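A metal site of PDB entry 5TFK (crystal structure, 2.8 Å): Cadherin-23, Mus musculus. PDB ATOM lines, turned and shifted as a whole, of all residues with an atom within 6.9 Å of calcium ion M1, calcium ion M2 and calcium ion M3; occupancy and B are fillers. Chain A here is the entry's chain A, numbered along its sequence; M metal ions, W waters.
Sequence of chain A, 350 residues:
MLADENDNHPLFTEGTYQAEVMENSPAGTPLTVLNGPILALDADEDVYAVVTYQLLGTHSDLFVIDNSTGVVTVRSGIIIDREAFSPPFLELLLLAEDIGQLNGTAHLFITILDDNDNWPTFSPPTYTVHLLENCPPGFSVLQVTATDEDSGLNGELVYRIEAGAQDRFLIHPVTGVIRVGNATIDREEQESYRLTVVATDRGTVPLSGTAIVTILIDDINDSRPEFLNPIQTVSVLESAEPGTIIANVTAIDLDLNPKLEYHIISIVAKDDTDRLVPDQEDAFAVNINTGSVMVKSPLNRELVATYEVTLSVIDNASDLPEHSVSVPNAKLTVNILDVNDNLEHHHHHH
O of Ser 324 lies within hydrogen-bond range of N of Asp 315, at 3.0 Å. ND1 of His 323 is in hydrogen-bond range of O of Asp 222 (2.7 Å). The side-chain amide nitrogen of Asn 221 is in hydrogen-bond range of the backbone carbonyl oxygen of Ala 317, at 3.5 Å. The side-chain carboxylate (OD2) of Asp 219 lies within hydrogen-bond range of the backbone NH (N) of Leu 256 (3.4 Å). The side-chain carboxylate (OE1) of Glu 188 lies close to the guanidinium group (NH2) of Arg 187 (3.0 Å). OD2 of Asp 222 lies close to ND2 of Asn 134, at 2.8 Å. OE1 of Glu 133 lies close to N of Arg 187, at 3.2 Å. The side-chain carboxylate of Asp 319 is in hydrogen-bond range of the backbone NH of Asn 221 (3.0 Å).
Four residues have an atom within 4 Å of calcium ion M1: Glu 133, Asp 186, Glu 188 and Asp 222.
Six residues have an atom within 4 Å of calcium ion M2: Glu 133, Glu 188, Asp 219, Ile 220, Asp 222 and Asp 255.
Of the 27 residues printed, 5 come within 4 Å of calcium ion M3. The nearest printed residue that does not touch calcium ion M3 is His 323 (4.1 Å).
Calcium ion M1 is bound by water W1 (2.2 Å), OD1 of Asp 186 (2.2 Å), OE2 of Glu 188 (2.3 Å), OD1 of Asp 222 (2.4 Å), OD2 of Asp 222 (2.5 Å) and OE1 of Glu 133 (2.5 Å).
Calcium ion M2 is bound by OE2 of Glu 188 (2.2 Å), O of Ile 220 (2.3 Å), OD1 of Asp 255 (2.3 Å), OD1 of Asp 219 (2.3 Å), OE2 of Glu 133 (2.3 Å), OD1 of Asp 222 (2.6 Å) and OE1 of Glu 188 (2.8 Å).
Calcium ion M3 is bound by O of Ser 223 (2.1 Å), OD2 of Asp 315 (2.4 Å), OD1 of Asp 253 (2.4 Å), OD1 of Asn 221 (2.5 Å), OD2 of Asp 253 (2.6 Å) and OD2 of Asp 255 (2.6 Å).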
ATOM      1  N   GLU A 133     -14.465 -15.333 -29.832  1.00  0.00           N
ATOM      2  CA  GLU A 133     -13.479 -16.161 -29.111  1.00  0.00           C
ATOM      3  C   GLU A 133     -14.023 -16.956 -27.905  1.00  0.00           C
ATOM      4  O   GLU A 133     -15.152 -16.728 -27.417  1.00  0.00           O
ATOM      5  CB  GLU A 133     -12.243 -15.332 -28.680  1.00  0.00           C
ATOM      6  CG  GLU A 133     -12.455 -14.328 -27.537  1.00  0.00           C
ATOM      7  CD  GLU A 133     -11.172 -13.697 -27.001  1.00  0.00           C
ATOM      8  OE1 GLU A 133     -10.235 -14.424 -26.622  1.00  0.00           O
ATOM      9  OE2 GLU A 133     -11.109 -12.465 -26.886  1.00  0.00           O
ATOM     10  N   ASN A 134     -13.178 -17.892 -27.437  1.00  0.00           N
ATOM     11  CA  ASN A 134     -13.507 -18.854 -26.365  1.00  0.00           C
ATOM     12  C   ASN A 134     -14.732 -19.698 -26.706  1.00  0.00           C
ATOM     13  O   ASN A 134     -15.658 -19.861 -25.920  1.00  0.00           O
ATOM     14  CB  ASN A 134     -13.751 -18.130 -25.034  1.00  0.00           C
ATOM     15  CG  ASN A 134     -12.592 -17.278 -24.625  1.00  0.00           C
ATOM     16  OD1 ASN A 134     -11.461 -17.752 -24.603  1.00  0.00           O
ATOM     17  ND2 ASN A 134     -12.869 -16.021 -24.302  1.00  0.00           N
ATOM     18  N   ILE A 185      -9.823 -21.042 -29.097  1.00  0.00           N
ATOM     19  CA  ILE A 185      -9.678 -19.878 -29.964  1.00  0.00           C
ATOM     20  C   ILE A 185      -9.519 -18.642 -29.128  1.00  0.00           C
ATOM     21  O   ILE A 185     -10.507 -18.104 -28.628  1.00  0.00           O
ATOM     22  CB  ILE A 185     -10.911 -19.696 -30.869  1.00  0.00           C
ATOM     23  CG1 ILE A 185     -11.052 -20.894 -31.819  1.00  0.00           C
ATOM     24  CG2 ILE A 185     -10.873 -18.382 -31.652  1.00  0.00           C
ATOM     25  CD1 ILE A 185      -9.767 -21.315 -32.510  1.00  0.00           C
ATOM     26  N   ASP A 186      -8.273 -18.203 -28.957  1.00  0.00           N
ATOM     27  CA  ASP A 186      -7.967 -17.003 -28.179  1.00  0.00           C
ATOM     28  C   ASP A 186      -7.605 -15.902 -29.141  1.00  0.00           C
ATOM     29  O   ASP A 186      -6.597 -16.017 -29.826  1.00  0.00           O
ATOM     30  CB  ASP A 186      -6.767 -17.287 -27.271  1.00  0.00           C
ATOM     31  CG  ASP A 186      -6.457 -16.142 -26.324  1.00  0.00           C
ATOM     32  OD1 ASP A 186      -7.192 -15.145 -26.298  1.00  0.00           O
ATOM     33  OD2 ASP A 186      -5.451 -16.264 -25.586  1.00  0.00           O
ATOM     34  N   ARG A 187      -8.416 -14.849 -29.174  1.00  0.00           N
ATOM     35  CA  ARG A 187      -8.119 -13.668 -29.990  1.00  0.00           C
ATOM     36  C   ARG A 187      -6.768 -13.040 -29.702  1.00  0.00           C
ATOM     37  O   ARG A 187      -6.150 -12.468 -30.597  1.00  0.00           O
ATOM     38  CB  ARG A 187      -9.166 -12.580 -29.780  1.00  0.00           C
ATOM     39  CG  ARG A 187      -9.271 -11.613 -30.955  1.00  0.00           C
ATOM     40  CD  ARG A 187      -9.951 -10.328 -30.555  1.00  0.00           C
ATOM     41  NE  ARG A 187      -9.061  -9.606 -29.655  1.00  0.00           N
ATOM     42  CZ  ARG A 187      -8.133  -8.741 -30.033  1.00  0.00           C
ATOM     43  NH1 ARG A 187      -7.989  -8.387 -31.313  1.00  0.00           N
ATOM     44  NH2 ARG A 187      -7.375  -8.180 -29.096  1.00  0.00           N
ATOM     45  N   GLU A 188      -6.329 -13.114 -28.455  1.00  0.00           N
ATOM     46  CA  GLU A 188      -5.015 -12.598 -28.071  1.00  0.00           C
ATOM     47  C   GLU A 188      -3.859 -13.477 -28.598  1.00  0.00           C
ATOM     48  O   GLU A 188      -2.737 -12.991 -28.735  1.00  0.00           O
ATOM     49  CB  GLU A 188      -4.937 -12.441 -26.555  1.00  0.00           C
ATOM     50  CG  GLU A 188      -5.605 -11.185 -26.001  1.00  0.00           C
ATOM     51  CD  GLU A 188      -7.110 -11.137 -26.189  1.00  0.00           C
ATOM     52  OE1 GLU A 188      -7.617 -10.380 -27.054  1.00  0.00           O
ATOM     53  OE2 GLU A 188      -7.824 -11.841 -25.446  1.00  0.00           O
ATOM     54  N   GLU A 189      -4.136 -14.747 -28.885  1.00  0.00           N
ATOM     55  CA  GLU A 189      -3.157 -15.624 -29.552  1.00  0.00           C
ATOM     56  C   GLU A 189      -3.086 -15.340 -31.050  1.00  0.00           C
ATOM     57  O   GLU A 189      -2.011 -15.299 -31.642  1.00  0.00           O
ATOM     58  CB  GLU A 189      -3.484 -17.115 -29.317  1.00  0.00           C
ATOM     59  CG  GLU A 189      -2.547 -18.080 -30.038  1.00  0.00           C
ATOM     60  CD  GLU A 189      -2.636 -19.498 -29.525  1.00  0.00           C
ATOM     61  OE1 GLU A 189      -1.576 -20.131 -29.370  1.00  0.00           O
ATOM     62  OE2 GLU A 189      -3.767 -19.987 -29.300  1.00  0.00           O
ATOM     63  N   ASP A 218     -13.692 -12.090 -32.740  1.00  0.00           N
ATOM     64  CA  ASP A 218     -14.237 -10.946 -32.070  1.00  0.00           C
ATOM     65  C   ASP A 218     -13.771 -11.099 -30.653  1.00  0.00           C
ATOM     66  O   ASP A 218     -13.463 -12.206 -30.201  1.00  0.00           O
ATOM     67  CB  ASP A 218     -15.756 -10.917 -32.184  1.00  0.00           C
ATOM     68  CG  ASP A 218     -16.209 -10.449 -33.535  1.00  0.00           C
ATOM     69  OD1 ASP A 218     -15.335 -10.138 -34.367  1.00  0.00           O
ATOM     70  OD2 ASP A 218     -17.421 -10.379 -33.790  1.00  0.00           O
ATOM     71  N   ASP A 219     -13.680  -9.985 -29.947  1.00  0.00           N
ATOM     72  CA  ASP A 219     -13.052  -9.944 -28.619  1.00  0.00           C
ATOM     73  C   ASP A 219     -14.077 -10.114 -27.497  1.00  0.00           C
ATOM     74  O   ASP A 219     -15.150  -9.514 -27.515  1.00  0.00           O
ATOM     75  CB  ASP A 219     -12.303  -8.637 -28.466  1.00  0.00           C
ATOM     76  CG  ASP A 219     -11.513  -8.564 -27.201  1.00  0.00           C
ATOM     77  OD1 ASP A 219     -10.563  -9.352 -27.027  1.00  0.00           O
ATOM     78  OD2 ASP A 219     -11.862  -7.704 -26.368  1.00  0.00           O
ATOM     79  N   ILE A 220     -13.748 -11.015 -26.578  1.00  0.00           N
ATOM     80  CA  ILE A 220     -14.252 -10.919 -25.226  1.00  0.00           C
ATOM     81  C   ILE A 220     -13.079 -10.332 -24.431  1.00  0.00           C
ATOM     82  O   ILE A 220     -11.922 -10.676 -24.677  1.00  0.00           O
ATOM     83  CB  ILE A 220     -14.660 -12.297 -24.656  1.00  0.00           C
ATOM     84  CG1 ILE A 220     -15.734 -12.972 -25.523  1.00  0.00           C
ATOM     85  CG2 ILE A 220     -15.188 -12.133 -23.243  1.00  0.00           C
ATOM     86  CD1 ILE A 220     -15.938 -14.455 -25.213  1.00  0.00           C
ATOM     87  N   ASN A 221     -13.386  -9.416 -23.508  1.00  0.00           N
ATOM     88  CA  ASN A 221     -12.377  -8.883 -22.593  1.00  0.00           C
ATOM     89  C   ASN A 221     -12.056  -9.919 -21.518  1.00  0.00           C
ATOM     90  O   ASN A 221     -12.619  -9.907 -20.422  1.00  0.00           O
ATOM     91  CB  ASN A 221     -12.849  -7.574 -21.969  1.00  0.00           C
ATOM     92  CG  ASN A 221     -11.743  -6.855 -21.245  1.00  0.00           C
ATOM     93  OD1 ASN A 221     -11.038  -7.452 -20.432  1.00  0.00           O
ATOM     94  ND2 ASN A 221     -11.563  -5.582 -21.545  1.00  0.00           N
ATOM     95  N   ASP A 222     -11.165 -10.836 -21.848  1.00  0.00           N
ATOM     96  CA  ASP A 222     -10.961 -12.029 -21.061  1.00  0.00           C
ATOM     97  C   ASP A 222      -9.534 -12.159 -20.604  1.00  0.00           C
ATOM     98  O   ASP A 222      -9.145 -13.199 -20.091  1.00  0.00           O
ATOM     99  CB  ASP A 222     -11.367 -13.273 -21.884  1.00  0.00           C
ATOM    100  CG  ASP A 222     -10.480 -13.489 -23.107  1.00  0.00           C
ATOM    101  OD1 ASP A 222      -9.785 -12.560 -23.559  1.00  0.00           O
ATOM    102  OD2 ASP A 222     -10.511 -14.603 -23.637  1.00  0.00           O
ATOM    103  N   SER A 223      -8.765 -11.089 -20.760  1.00  0.00           N
ATOM    104  CA  SER A 223      -7.327 -11.157 -20.582  1.00  0.00           C
ATOM    105  C   SER A 223      -6.934 -10.187 -19.477  1.00  0.00           C
ATOM    106  O   SER A 223      -7.256  -9.002 -19.555  1.00  0.00           O
ATOM    107  CB  SER A 223      -6.627 -10.792 -21.881  1.00  0.00           C
ATOM    108  OG  SER A 223      -5.344 -11.351 -21.929  1.00  0.00           O
ATOM    109  N   ARG A 224      -6.289 -10.712 -18.434  1.00  0.00           N
ATOM    110  CA  ARG A 224      -5.964  -9.925 -17.251  1.00  0.00           C
ATOM    111  C   ARG A 224      -4.802  -8.955 -17.493  1.00  0.00           C
ATOM    112  O   ARG A 224      -3.817  -9.303 -18.142  1.00  0.00           O
ATOM    113  CB  ARG A 224      -5.667 -10.821 -16.039  1.00  0.00           C
ATOM    114  CG  ARG A 224      -4.257 -11.409 -15.987  1.00  0.00           C
ATOM    115  CD  ARG A 224      -3.953 -12.072 -14.647  1.00  0.00           C
ATOM    116  NE  ARG A 224      -4.584 -13.385 -14.470  1.00  0.00           N
ATOM    117  CZ  ARG A 224      -5.724 -13.612 -13.830  1.00  0.00           C
ATOM    118  NH1 ARG A 224      -6.438 -12.624 -13.300  1.00  0.00           N
ATOM    119  NH2 ARG A 224      -6.175 -14.859 -13.732  1.00  0.00           N
ATOM    120  N   PRO A 225      -4.896  -7.754 -16.924  1.00  0.00           N
ATOM    121  CA  PRO A 225      -3.749  -6.849 -17.009  1.00  0.00           C
ATOM    122  C   PRO A 225      -2.501  -7.415 -16.341  1.00  0.00           C
ATOM    123  O   PRO A 225      -2.542  -8.113 -15.304  1.00  0.00           O
ATOM    124  CB  PRO A 225      -4.255  -5.569 -16.322  1.00  0.00           C
ATOM    125  CG  PRO A 225      -5.400  -5.979 -15.473  1.00  0.00           C
ATOM    126  CD  PRO A 225      -5.994  -7.176 -16.135  1.00  0.00           C
ATOM    127  N   ASP A 253      -2.731  -4.549 -21.095  1.00  0.00           N
ATOM    128  CA  ASP A 253      -3.901  -5.418 -21.308  1.00  0.00           C
ATOM    129  C   ASP A 253      -4.154  -5.611 -22.812  1.00  0.00           C
ATOM    130  O   ASP A 253      -4.245  -4.655 -23.542  1.00  0.00           O
ATOM    131  CB  ASP A 253      -5.144  -4.787 -20.668  1.00  0.00           C
ATOM    132  CG  ASP A 253      -6.245  -5.807 -20.319  1.00  0.00           C
ATOM    133  OD1 ASP A 253      -6.979  -6.289 -21.197  1.00  0.00           O
ATOM    134  OD2 ASP A 253      -6.443  -6.053 -19.117  1.00  0.00           O
ATOM    135  N   LEU A 254      -4.206  -6.865 -23.238  1.00  0.00           N
ATOM    136  CA  LEU A 254      -4.177  -7.201 -24.651  1.00  0.00           C
ATOM    137  C   LEU A 254      -5.563  -7.283 -25.284  1.00  0.00           C
ATOM    138  O   LEU A 254      -5.678  -7.549 -26.472  1.00  0.00           O
ATOM    139  CB  LEU A 254      -3.448  -8.527 -24.856  1.00  0.00           C
ATOM    140  CG  LEU A 254      -2.009  -8.545 -24.341  1.00  0.00           C
ATOM    141  CD1 LEU A 254      -1.518  -9.978 -24.141  1.00  0.00           C
ATOM    142  CD2 LEU A 254      -1.109  -7.767 -25.284  1.00  0.00           C
ATOM    143  N   ASP A 255      -6.615  -7.035 -24.507  1.00  0.00           N
ATOM    144  CA  ASP A 255      -7.965  -6.968 -25.040  1.00  0.00           C
ATOM    145  C   ASP A 255      -8.178  -5.640 -25.754  1.00  0.00           C
ATOM    146  O   ASP A 255      -7.315  -4.769 -25.715  1.00  0.00           O
ATOM    147  CB  ASP A 255      -9.001  -7.148 -23.918  1.00  0.00           C
ATOM    148  CG  ASP A 255      -8.957  -8.528 -23.304  1.00  0.00           C
ATOM    149  OD1 ASP A 255      -9.052  -9.529 -24.056  1.00  0.00           O
ATOM    150  OD2 ASP A 255      -8.848  -8.611 -22.052  1.00  0.00           O
ATOM    151  N   LEU A 256      -9.346  -5.477 -26.368  1.00  0.00           N
ATOM    152  CA  LEU A 256      -9.546  -4.422 -27.332  1.00  0.00           C
ATOM    153  C   LEU A 256      -9.766  -3.047 -26.727  1.00  0.00           C
ATOM    154  O   LEU A 256      -9.291  -2.076 -27.296  1.00  0.00           O
ATOM    155  CB  LEU A 256     -10.657  -4.771 -28.327  1.00  0.00           C
ATOM    156  CG  LEU A 256     -10.169  -5.419 -29.634  1.00  0.00           C
ATOM    157  CD1 LEU A 256     -11.321  -5.931 -30.475  1.00  0.00           C
ATOM    158  CD2 LEU A 256      -9.335  -4.462 -30.480  1.00  0.00           C
ATOM    159  N   PRO A 258      -9.460  -1.707 -22.994  1.00  0.00           N
ATOM    160  CA  PRO A 258      -9.309  -1.717 -21.545  1.00  0.00           C
ATOM    161  C   PRO A 258      -9.530  -0.340 -20.958  1.00  0.00           C
ATOM    162  O   PRO A 258      -9.309   0.665 -21.636  1.00  0.00           O
ATOM    163  CB  PRO A 258      -7.861  -2.162 -21.341  1.00  0.00           C
ATOM    164  CG  PRO A 258      -7.191  -1.977 -22.645  1.00  0.00           C
ATOM    165  CD  PRO A 258      -8.243  -2.157 -23.684  1.00  0.00           C
ATOM    166  N   LEU A 260      -7.798   0.771 -17.567  1.00  0.00           N
ATOM    167  CA  LEU A 260      -6.928   0.332 -16.505  1.00  0.00           C
ATOM    168  C   LEU A 260      -6.940   1.355 -15.366  1.00  0.00           C
ATOM    169  O   LEU A 260      -6.768   2.560 -15.586  1.00  0.00           O
ATOM    170  CB  LEU A 260      -5.511   0.120 -17.019  1.00  0.00           C
ATOM    171  CG  LEU A 260      -5.311  -0.992 -18.067  1.00  0.00           C
ATOM    172  CD1 LEU A 260      -3.831  -1.286 -18.315  1.00  0.00           C
ATOM    173  CD2 LEU A 260      -6.005  -2.264 -17.656  1.00  0.00           C
ATOM    174  N   ASP A 315      -8.728  -4.031 -14.947  1.00  0.00           N
ATOM    175  CA  ASP A 315      -9.459  -3.648 -16.169  1.00  0.00           C
ATOM    176  C   ASP A 315     -10.942  -3.492 -15.860  1.00  0.00           C
ATOM    177  O   ASP A 315     -11.552  -4.463 -15.464  1.00  0.00           O
ATOM    178  CB  ASP A 315      -9.248  -4.751 -17.216  1.00  0.00           C
ATOM    179  CG  ASP A 315      -9.610  -4.309 -18.628  1.00  0.00           C
ATOM    180  OD1 ASP A 315     -10.230  -3.234 -18.774  1.00  0.00           O
ATOM    181  OD2 ASP A 315      -9.279  -5.047 -19.604  1.00  0.00           O
ATOM    182  N   ALA A 317     -13.250  -2.763 -17.916  1.00  0.00           N
ATOM    183  CA  ALA A 317     -14.027  -3.220 -19.039  1.00  0.00           C
ATOM    184  C   ALA A 317     -14.077  -4.738 -19.044  1.00  0.00           C
ATOM    185  O   ALA A 317     -14.639  -5.319 -19.972  1.00  0.00           O
ATOM    186  CB  ALA A 317     -13.425  -2.702 -20.323  1.00  0.00           C
ATOM    187  N   SER A 318     -13.537  -5.390 -18.031  1.00  0.00           N
ATOM    188  CA  SER A 318     -13.406  -6.845 -18.080  1.00  0.00           C
ATOM    189  C   SER A 318     -14.770  -7.520 -18.105  1.00  0.00           C
ATOM    190  O   SER A 318     -15.725  -7.055 -17.475  1.00  0.00           O
ATOM    191  CB  SER A 318     -12.538  -7.360 -16.932  1.00  0.00           C
ATOM    192  OG  SER A 318     -11.837  -8.540 -17.318  1.00  0.00           O
ATOM    193  N   ASP A 319     -14.857  -8.571 -18.916  1.00  0.00           N
ATOM    194  CA  ASP A 319     -16.115  -9.274 -19.147  1.00  0.00           C
ATOM    195  C   ASP A 319     -16.199 -10.507 -18.261  1.00  0.00           C
ATOM    196  O   ASP A 319     -17.284 -10.987 -17.975  1.00  0.00           O
ATOM    197  CB  ASP A 319     -16.260  -9.667 -20.620  1.00  0.00           C
ATOM    198  CG  ASP A 319     -16.645  -8.489 -21.526  1.00  0.00           C
ATOM    199  OD1 ASP A 319     -17.702  -7.841 -21.290  1.00  0.00           O
ATOM    200  OD2 ASP A 319     -15.910  -8.219 -22.499  1.00  0.00           O
ATOM    201  N   HIS A 323     -10.526 -12.657 -14.698  1.00  0.00           N
ATOM    202  CA  HIS A 323      -9.363 -12.206 -15.492  1.00  0.00           C
ATOM    203  C   HIS A 323      -9.307 -10.670 -15.572  1.00  0.00           C
ATOM    204  O   HIS A 323      -9.071 -10.074 -16.647  1.00  0.00           O
ATOM    205  CB  HIS A 323      -9.414 -12.782 -16.913  1.00  0.00           C
ATOM    206  CG  HIS A 323      -9.172 -14.255 -16.994  1.00  0.00           C
ATOM    207  ND1 HIS A 323      -9.441 -15.001 -18.123  1.00  0.00           N
ATOM    208  CD2 HIS A 323      -8.686 -15.131 -16.081  1.00  0.00           C
ATOM    209  CE1 HIS A 323      -9.131 -16.262 -17.908  1.00  0.00           C
ATOM    210  NE2 HIS A 323      -8.668 -16.373 -16.678  1.00  0.00           N
ATOM    211  N   SER A 324      -9.545 -10.033 -14.431  1.00  0.00           N
ATOM    212  CA  SER A 324      -9.737  -8.593 -14.414  1.00  0.00           C
ATOM    213  C   SER A 324      -8.794  -7.856 -13.493  1.00  0.00           C
ATOM    214  O   SER A 324      -8.737  -6.653 -13.578  1.00  0.00           O
ATOM    215  CB  SER A 324     -11.174  -8.257 -14.014  1.00  0.00           C
ATOM    216  OG  SER A 324     -11.363  -8.498 -12.650  1.00  0.00           O
HETATM  217 CA    CA M   1      -8.446 -14.036 -24.900  1.00  0.00          CA
HETATM  218 CA    CA M   2      -9.884 -11.003 -25.587  1.00  0.00          CA
HETATM  219 CA    CA M   3      -8.605  -7.364 -19.743  1.00  0.00          CA
HETATM  220  O   HOH W   1      -9.395 -15.933 -25.258  1.00  0.00           O
